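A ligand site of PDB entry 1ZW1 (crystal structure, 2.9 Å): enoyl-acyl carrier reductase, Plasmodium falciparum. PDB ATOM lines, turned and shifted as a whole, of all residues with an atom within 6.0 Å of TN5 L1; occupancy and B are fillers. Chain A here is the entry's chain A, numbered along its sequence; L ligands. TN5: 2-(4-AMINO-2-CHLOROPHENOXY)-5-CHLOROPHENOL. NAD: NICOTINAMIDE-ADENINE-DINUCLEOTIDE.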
ATOM      1  N   LEU A 120      -6.213   3.452 -27.448  1.00  0.00           N
ATOM      2  CA  LEU A 120      -5.351   4.546 -27.028  1.00  0.00           C
ATOM      3  C   LEU A 120      -5.018   4.585 -25.537  1.00  0.00           C
ATOM      4  O   LEU A 120      -5.863   4.289 -24.698  1.00  0.00           O
ATOM      5  CB  LEU A 120      -5.997   5.869 -27.429  1.00  0.00           C
ATOM      6  CG  LEU A 120      -7.330   6.179 -26.733  1.00  0.00           C
ATOM      7  CD1 LEU A 120      -7.073   6.902 -25.403  1.00  0.00           C
ATOM      8  CD2 LEU A 120      -8.209   7.019 -27.659  1.00  0.00           C
ATOM      9  N   ALA A 121      -3.786   4.984 -25.222  1.00  0.00           N
ATOM     10  CA  ALA A 121      -3.351   5.089 -23.838  1.00  0.00           C
ATOM     11  C   ALA A 121      -2.191   6.059 -23.680  1.00  0.00           C
ATOM     12  O   ALA A 121      -1.539   6.446 -24.655  1.00  0.00           O
ATOM     13  CB  ALA A 121      -2.964   3.728 -23.326  1.00  0.00           C
ATOM     14  N   ASN A 122      -1.938   6.460 -22.439  1.00  0.00           N
ATOM     15  CA  ASN A 122      -0.831   7.360 -22.124  1.00  0.00           C
ATOM     16  C   ASN A 122      -0.690   7.607 -20.631  1.00  0.00           C
ATOM     17  O   ASN A 122      -1.626   8.045 -19.968  1.00  0.00           O
ATOM     18  CB  ASN A 122      -0.955   8.694 -22.846  1.00  0.00           C
ATOM     19  CG  ASN A 122       0.302   9.540 -22.728  1.00  0.00           C
ATOM     20  OD1 ASN A 122       1.354   9.194 -23.264  1.00  0.00           O
ATOM     21  ND2 ASN A 122       0.216  10.645 -22.006  1.00  0.00           N
ATOM     22  N   ALA A 123       0.504   7.312 -20.123  1.00  0.00           N
ATOM     23  CA  ALA A 123       0.835   7.504 -18.719  1.00  0.00           C
ATOM     24  C   ALA A 123       2.142   8.302 -18.662  1.00  0.00           C
ATOM     25  O   ALA A 123       3.247   7.736 -18.755  1.00  0.00           O
ATOM     26  CB  ALA A 123       0.994   6.167 -18.031  1.00  0.00           C
ATOM     27  N   LYS A 124       2.008   9.624 -18.503  1.00  0.00           N
ATOM     28  CA  LYS A 124       3.128  10.545 -18.430  1.00  0.00           C
ATOM     29  C   LYS A 124       4.282  10.158 -17.509  1.00  0.00           C
ATOM     30  O   LYS A 124       5.394  10.632 -17.693  1.00  0.00           O
ATOM     31  CB  LYS A 124       2.629  11.939 -18.070  1.00  0.00           C
ATOM     32  CG  LYS A 124       1.862  12.629 -19.184  1.00  0.00           C
ATOM     33  CD  LYS A 124       1.259  13.963 -18.746  1.00  0.00           C
ATOM     34  CE  LYS A 124       0.511  14.637 -19.897  1.00  0.00           C
ATOM     35  NZ  LYS A 124      -0.325  15.813 -19.471  1.00  0.00           N
ATOM     36  N   VAL A 126       4.966   6.754 -16.715  1.00  0.00           N
ATOM     37  CA  VAL A 126       5.145   5.316 -16.852  1.00  0.00           C
ATOM     38  C   VAL A 126       6.504   4.814 -16.359  1.00  0.00           C
ATOM     39  O   VAL A 126       6.606   3.682 -15.882  1.00  0.00           O
ATOM     40  CB  VAL A 126       4.953   4.861 -18.314  1.00  0.00           C
ATOM     41  CG1 VAL A 126       6.068   5.402 -19.190  1.00  0.00           C
ATOM     42  CG2 VAL A 126       4.905   3.351 -18.383  1.00  0.00           C
ATOM     43  N   THR A 170      -6.421  -3.816 -23.450  1.00  0.00           N
ATOM     44  CA  THR A 170      -5.909  -3.704 -22.095  1.00  0.00           C
ATOM     45  C   THR A 170      -4.672  -4.593 -21.880  1.00  0.00           C
ATOM     46  O   THR A 170      -4.289  -5.373 -22.760  1.00  0.00           O
ATOM     47  CB  THR A 170      -7.064  -4.033 -21.092  1.00  0.00           C
ATOM     48  OG1 THR A 170      -6.648  -3.743 -19.759  1.00  0.00           O
ATOM     49  CG2 THR A 170      -7.500  -5.497 -21.225  1.00  0.00           C
ATOM     50  N   TYR A 171      -4.035  -4.461 -20.708  1.00  0.00           N
ATOM     51  CA  TYR A 171      -2.824  -5.233 -20.452  1.00  0.00           C
ATOM     52  C   TYR A 171      -2.867  -5.997 -19.131  1.00  0.00           C
ATOM     53  O   TYR A 171      -3.239  -5.455 -18.087  1.00  0.00           O
ATOM     54  CB  TYR A 171      -1.601  -4.303 -20.525  1.00  0.00           C
ATOM     55  CG  TYR A 171      -0.264  -5.006 -20.474  1.00  0.00           C
ATOM     56  CD1 TYR A 171      -0.002  -6.121 -21.269  1.00  0.00           C
ATOM     57  CD2 TYR A 171       0.732  -4.586 -19.590  1.00  0.00           C
ATOM     58  CE1 TYR A 171       1.193  -6.804 -21.181  1.00  0.00           C
ATOM     59  CE2 TYR A 171       1.953  -5.270 -19.487  1.00  0.00           C
ATOM     60  CZ  TYR A 171       2.158  -6.381 -20.282  1.00  0.00           C
ATOM     61  OH  TYR A 171       3.322  -7.109 -20.156  1.00  0.00           O
ATOM     62  N   TYR A 181       5.802  -1.318 -15.619  1.00  0.00           N
ATOM     63  CA  TYR A 181       4.588  -0.840 -16.260  1.00  0.00           C
ATOM     64  C   TYR A 181       3.978   0.091 -15.239  1.00  0.00           C
ATOM     65  O   TYR A 181       2.916  -0.187 -14.690  1.00  0.00           O
ATOM     66  CB  TYR A 181       3.641  -2.015 -16.507  1.00  0.00           C
ATOM     67  CG  TYR A 181       2.469  -1.703 -17.398  1.00  0.00           C
ATOM     68  CD1 TYR A 181       2.633  -1.462 -18.760  1.00  0.00           C
ATOM     69  CD2 TYR A 181       1.180  -1.650 -16.878  1.00  0.00           C
ATOM     70  CE1 TYR A 181       1.539  -1.190 -19.576  1.00  0.00           C
ATOM     71  CE2 TYR A 181       0.076  -1.384 -17.685  1.00  0.00           C
ATOM     72  CZ  TYR A 181       0.259  -1.151 -19.033  1.00  0.00           C
ATOM     73  OH  TYR A 181      -0.843  -0.907 -19.819  1.00  0.00           O
ATOM     74  N   MET A 185      -0.370   3.026 -15.277  1.00  0.00           N
ATOM     75  CA  MET A 185      -0.892   2.191 -16.362  1.00  0.00           C
ATOM     76  C   MET A 185      -1.474   0.863 -15.845  1.00  0.00           C
ATOM     77  O   MET A 185      -2.314   0.258 -16.504  1.00  0.00           O
ATOM     78  CB  MET A 185       0.170   1.880 -17.425  1.00  0.00           C
ATOM     79  CG  MET A 185       0.181   2.849 -18.628  1.00  0.00           C
ATOM     80  SD  MET A 185      -1.438   3.225 -19.350  1.00  0.00           S
ATOM     81  CE  MET A 185      -1.996   1.624 -19.680  1.00  0.00           C
ATOM     82  N   LYS A 189      -5.427   0.341 -16.502  1.00  0.00           N
ATOM     83  CA  LYS A 189      -5.944  -0.860 -17.146  1.00  0.00           C
ATOM     84  C   LYS A 189      -6.857  -1.688 -16.246  1.00  0.00           C
ATOM     85  O   LYS A 189      -7.835  -2.283 -16.715  1.00  0.00           O
ATOM     86  CB  LYS A 189      -4.786  -1.704 -17.655  1.00  0.00           C
ATOM     87  CG  LYS A 189      -3.989  -1.034 -18.760  1.00  0.00           C
ATOM     88  CD  LYS A 189      -4.864  -0.613 -19.921  1.00  0.00           C
ATOM     89  CE  LYS A 189      -3.994  -0.337 -21.140  1.00  0.00           C
ATOM     90  NZ  LYS A 189      -4.752   0.066 -22.363  1.00  0.00           N
ATOM     91  N   GLY A 217      -0.776  -8.962 -26.014  1.00  0.00           N
ATOM     92  CA  GLY A 217       0.547  -9.254 -25.505  1.00  0.00           C
ATOM     93  C   GLY A 217       1.484  -8.198 -26.045  1.00  0.00           C
ATOM     94  O   GLY A 217       1.033  -7.239 -26.673  1.00  0.00           O
ATOM     95  N   PRO A 218       2.802  -8.343 -25.868  1.00  0.00           N
ATOM     96  CA  PRO A 218       3.804  -7.390 -26.332  1.00  0.00           C
ATOM     97  C   PRO A 218       3.761  -7.071 -27.832  1.00  0.00           C
ATOM     98  O   PRO A 218       3.553  -7.955 -28.671  1.00  0.00           O
ATOM     99  CB  PRO A 218       5.133  -8.070 -25.959  1.00  0.00           C
ATOM    100  CG  PRO A 218       4.758  -9.097 -24.934  1.00  0.00           C
ATOM    101  CD  PRO A 218       3.457  -9.602 -25.448  1.00  0.00           C
ATOM    102  N   LEU A 219       3.962  -5.804 -28.164  1.00  0.00           N
ATOM    103  CA  LEU A 219       3.996  -5.332 -29.536  1.00  0.00           C
ATOM    104  C   LEU A 219       4.900  -4.105 -29.612  1.00  0.00           C
ATOM    105  O   LEU A 219       4.710  -3.147 -28.859  1.00  0.00           O
ATOM    106  CB  LEU A 219       2.598  -4.955 -30.030  1.00  0.00           C
ATOM    107  CG  LEU A 219       2.605  -4.661 -31.541  1.00  0.00           C
ATOM    108  CD1 LEU A 219       3.031  -5.931 -32.273  1.00  0.00           C
ATOM    109  CD2 LEU A 219       1.242  -4.188 -32.023  1.00  0.00           C
ATOM    110  N   SER A 221       5.404  -1.126 -30.764  1.00  0.00           N
ATOM    111  CA  SER A 221       4.712   0.026 -31.317  1.00  0.00           C
ATOM    112  C   SER A 221       5.433   1.250 -30.764  1.00  0.00           C
ATOM    113  O   SER A 221       6.261   1.095 -29.884  1.00  0.00           O
ATOM    114  CB  SER A 221       3.262   0.014 -30.851  1.00  0.00           C
ATOM    115  OG  SER A 221       3.190  -0.142 -29.448  1.00  0.00           O
ATOM    116  N   ALA A 223       4.416   3.533 -28.779  1.00  0.00           N
ATOM    117  CA  ALA A 223       4.107   3.654 -27.363  1.00  0.00           C
ATOM    118  C   ALA A 223       4.941   2.680 -26.541  1.00  0.00           C
ATOM    119  O   ALA A 223       5.497   3.036 -25.503  1.00  0.00           O
ATOM    120  CB  ALA A 223       2.641   3.402 -27.144  1.00  0.00           C
ATOM    121  N   ALA A 224       5.021   1.440 -27.026  1.00  0.00           N
ATOM    122  CA  ALA A 224       5.788   0.412 -26.344  1.00  0.00           C
ATOM    123  C   ALA A 224       7.272   0.775 -26.312  1.00  0.00           C
ATOM    124  O   ALA A 224       7.924   0.618 -25.288  1.00  0.00           O
ATOM    125  CB  ALA A 224       5.601  -0.918 -27.051  1.00  0.00           C
ATOM    126  N   ILE A 227       8.000   3.656 -23.979  1.00  0.00           N
ATOM    127  CA  ILE A 227       7.936   3.394 -22.539  1.00  0.00           C
ATOM    128  C   ILE A 227       9.290   3.643 -21.864  1.00  0.00           C
ATOM    129  O   ILE A 227       9.401   4.515 -21.010  1.00  0.00           O
ATOM    130  CB  ILE A 227       7.497   1.948 -22.248  1.00  0.00           C
ATOM    131  CG1 ILE A 227       6.034   1.758 -22.669  1.00  0.00           C
ATOM    132  CG2 ILE A 227       7.682   1.637 -20.776  1.00  0.00           C
ATOM    133  CD1 ILE A 227       5.474   0.387 -22.349  1.00  0.00           C
ATOM    134  N   PHE A 272      11.917  -2.001 -21.884  1.00  0.00           N
ATOM    135  CA  PHE A 272      10.779  -2.733 -21.319  1.00  0.00           C
ATOM    136  C   PHE A 272      10.103  -3.611 -22.366  1.00  0.00           C
ATOM    137  O   PHE A 272       9.914  -4.810 -22.156  1.00  0.00           O
ATOM    138  CB  PHE A 272       9.758  -1.709 -20.805  1.00  0.00           C
ATOM    139  CG  PHE A 272       8.418  -2.295 -20.470  1.00  0.00           C
ATOM    140  CD1 PHE A 272       8.202  -2.947 -19.262  1.00  0.00           C
ATOM    141  CD2 PHE A 272       7.352  -2.184 -21.366  1.00  0.00           C
ATOM    142  CE1 PHE A 272       6.965  -3.479 -18.954  1.00  0.00           C
ATOM    143  CE2 PHE A 272       6.117  -2.716 -21.067  1.00  0.00           C
ATOM    144  CZ  PHE A 272       5.922  -3.363 -19.856  1.00  0.00           C
ATOM    145  N   ILE A 273       9.749  -2.985 -23.482  1.00  0.00           N
ATOM    146  CA  ILE A 273       9.079  -3.645 -24.587  1.00  0.00           C
ATOM    147  C   ILE A 273       9.895  -4.768 -25.212  1.00  0.00           C
ATOM    148  O   ILE A 273       9.353  -5.810 -25.582  1.00  0.00           O
ATOM    149  CB  ILE A 273       8.722  -2.620 -25.669  1.00  0.00           C
ATOM    150  CG1 ILE A 273       8.123  -3.331 -26.883  1.00  0.00           C
ATOM    151  CG2 ILE A 273       9.942  -1.812 -26.042  1.00  0.00           C
ATOM    152  CD1 ILE A 273       6.901  -4.133 -26.541  1.00  0.00           C
ATOM    153  N   ALA A 276       9.696  -7.754 -22.773  1.00  0.00           N
ATOM    154  CA  ALA A 276       8.417  -8.445 -22.728  1.00  0.00           C
ATOM    155  C   ALA A 276       8.275  -9.366 -23.941  1.00  0.00           C
ATOM    156  O   ALA A 276       7.846 -10.505 -23.822  1.00  0.00           O
ATOM    157  CB  ALA A 276       7.269  -7.436 -22.680  1.00  0.00           C
HETATM  158 CL13 TN5 L   1       3.557  -4.620 -22.752  1.00  0.00          CL
HETATM  159  C12 TN5 L   1       2.871  -3.216 -23.172  1.00  0.00           C
HETATM  160  C11 TN5 L   1       3.564  -2.350 -24.160  1.00  0.00           C
HETATM  161  C10 TN5 L   1       2.952  -1.017 -24.585  1.00  0.00           C
HETATM  162  C9  TN5 L   1       1.627  -0.575 -24.006  1.00  0.00           C
HETATM  163  C8  TN5 L   1       0.948  -1.457 -23.025  1.00  0.00           C
HETATM  164  O2  TN5 L   1      -0.242  -1.071 -22.503  1.00  0.00           O
HETATM  165  C7  TN5 L   1       1.568  -2.784 -22.599  1.00  0.00           C
HETATM  166  O1  TN5 L   1       1.081   0.667 -24.437  1.00  0.00           O
HETATM  167  C1  TN5 L   1       1.389   1.957 -23.790  1.00  0.00           C
HETATM  168  C6  TN5 L   1       2.312   2.208 -22.547  1.00  0.00           C
HETATM  169  C5  TN5 L   1       2.520   3.496 -22.037  1.00  0.00           C
HETATM  170  C4  TN5 L   1       1.903   4.685 -22.590  1.00  0.00           C
HETATM  171  N1  TN5 L   1       2.156   6.227 -21.962  1.00  0.00           N
HETATM  172  C3  TN5 L   1       0.949   4.564 -23.844  1.00  0.00           C
HETATM  173  C2  TN5 L   1       0.680   3.208 -24.452  1.00  0.00           C
HETATM  174 CL14 TN5 L   1      -0.327   3.053 -25.794  1.00  0.00          CL
HETATM  175  PA  NAD L   2      -0.083   3.186 -30.494  1.00  0.00           P
HETATM  176  O1A NAD L   2      -0.477   2.949 -31.926  1.00  0.00           O
HETATM  177  O2A NAD L   2       1.192   3.943 -30.217  1.00  0.00           O
HETATM  178  O5B NAD L   2      -1.395   3.947 -29.874  1.00  0.00           O
HETATM  179  C5B NAD L   2      -1.474   4.829 -28.736  1.00  0.00           C
HETATM  180  C4B NAD L   2      -2.349   5.989 -29.045  1.00  0.00           C
HETATM  181  O4B NAD L   2      -2.837   6.693 -27.874  1.00  0.00           O
HETATM  182  C3B NAD L   2      -1.619   7.062 -29.852  1.00  0.00           C
HETATM  183  O3B NAD L   2      -1.855   6.727 -31.245  1.00  0.00           O
HETATM  184  C2B NAD L   2      -2.240   8.399 -29.387  1.00  0.00           C
HETATM  185  O2B NAD L   2      -2.872   9.035 -30.478  1.00  0.00           O
HETATM  186  C1B NAD L   2      -3.256   7.989 -28.308  1.00  0.00           C
HETATM  187  N9A NAD L   2      -3.282   8.944 -27.154  1.00  0.00           N
HETATM  188  C8A NAD L   2      -2.611   9.300 -25.986  1.00  0.00           C
HETATM  189  N7A NAD L   2      -3.111  10.306 -25.286  1.00  0.00           N
HETATM  190  C5A NAD L   2      -4.233  10.674 -26.018  1.00  0.00           C
HETATM  191  C6A NAD L   2      -5.204  11.671 -25.830  1.00  0.00           C
HETATM  192  N6A NAD L   2      -5.186  12.499 -24.785  1.00  0.00           N
HETATM  193  N1A NAD L   2      -6.213  11.798 -26.758  1.00  0.00           N
HETATM  194  C2A NAD L   2      -6.260  10.964 -27.847  1.00  0.00           C
HETATM  195  N3A NAD L   2      -5.386   9.973 -28.143  1.00  0.00           N
HETATM  196  C4A NAD L   2      -4.367   9.860 -27.183  1.00  0.00           C
HETATM  197  O3  NAD L   2       0.186   1.980 -29.581  1.00  0.00           O
HETATM  198  PN  NAD L   2      -0.538   0.703 -29.221  1.00  0.00           P
HETATM  199  O1N NAD L   2      -0.965  -0.107 -30.393  1.00  0.00           O
HETATM  200  O2N NAD L   2       0.353   0.070 -28.221  1.00  0.00           O
HETATM  201  O5D NAD L   2      -1.680   1.196 -28.239  1.00  0.00           O
HETATM  202  C5D NAD L   2      -3.071   0.914 -28.401  1.00  0.00           C
HETATM  203  C4D NAD L   2      -3.619   0.206 -27.123  1.00  0.00           C
HETATM  204  O4D NAD L   2      -3.080  -1.165 -27.022  1.00  0.00           O
HETATM  205  C3D NAD L   2      -3.203   0.935 -25.838  1.00  0.00           C
HETATM  206  O3D NAD L   2      -4.321   1.194 -25.035  1.00  0.00           O
HETATM  207  C2D NAD L   2      -2.238   0.009 -25.220  1.00  0.00           C
HETATM  208  O2D NAD L   2      -2.115   0.156 -23.837  1.00  0.00           O
HETATM  209  C1D NAD L   2      -2.782  -1.318 -25.629  1.00  0.00           C
HETATM  210  N1N NAD L   2      -1.954  -2.490 -25.388  1.00  0.00           N
HETATM  211  C2N NAD L   2      -0.696  -2.574 -26.084  1.00  0.00           C
HETATM  212  C3N NAD L   2       0.254  -3.604 -25.991  1.00  0.00           C
HETATM  213  C7N NAD L   2       1.554  -3.706 -26.690  1.00  0.00           C
HETATM  214  O7N NAD L   2       2.382  -4.731 -26.505  1.00  0.00           O
HETATM  215  N7N NAD L   2       2.033  -2.811 -27.541  1.00  0.00           N
HETATM  216  C4N NAD L   2      -0.226  -4.583 -25.087  1.00  0.00           C
HETATM  217  C5N NAD L   2      -1.474  -4.612 -24.334  1.00  0.00           C
HETATM  218  C6N NAD L   2      -2.366  -3.483 -24.513  1.00  0.00           C
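An oxygen (O2) of TN5 L1 sits at hydrogen-bond distance from an oxygen (O2D) of NAD L2.
OH of Tyr 181 is in hydrogen-bond range of O2 of TN5 L1. An oxygen (O2N) of NAD L2 lies within hydrogen-bond range of the side-chain hydroxyl (OG) of Ser 221, 3.1 Å away. An oxygen (O4B) of NAD L2 lies within hydrogen-bond range of the backbone NH (N) of Ala 121 (3.3 Å). The backbone carbonyl oxygen of Leu 219 lies within hydrogen-bond range of a nitrogen (N7N) of NAD L2 (3.0 Å). The backbone NH (N) of Ala 123 lies close to a nitrogen (N1) of TN5 L1 (2.7 Å). O3D of NAD L2 sits at hydrogen-bond distance from O of Leu 120 (3.5 Å). N of Leu 219 sits at hydrogen-bond distance from O7N of NAD L2 (2.5 Å). N1 of TN5 L1 lies close to OD1 of Asn 122, at 3.3 Å. An oxygen (O3D) of NAD L2 is in hydrogen-bond range of the side-chain amino group of Lys 189, at 2.9 Å.
Merely in contact with TN5 L1: Ala 121 (3.2 Å), Ala 223 (3.3 Å), Tyr 171 (3.3 Å), Phe 272 (3.6 Å), Ala 224 (3.6 Å) and Ile 227 (3.7 Å). Hydrophobic or aromatic side chains within 4 Å of TN5 L1: Ala 121, Tyr 171, Tyr 181, Ala 223, Ala 224, Ile 227 and Phe 272. Nine residues have an atom within 4 Å of TN5 L1: Ala 121, Asn 122, Ala 123, Tyr 171, Tyr 181, Ala 223, Ala 224, Ile 227 and Phe 272. Along chain A the residues within 4 Å of TN5 L1 span positions 121 to 272. The nearest printed residue that does not touch TN5 L1 is Lys 189 (4.1 Å).
The backbone NH of Ala 224 is in hydrogen-bond range of the side-chain hydroxyl of Ser 221, at 3.4 Å.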
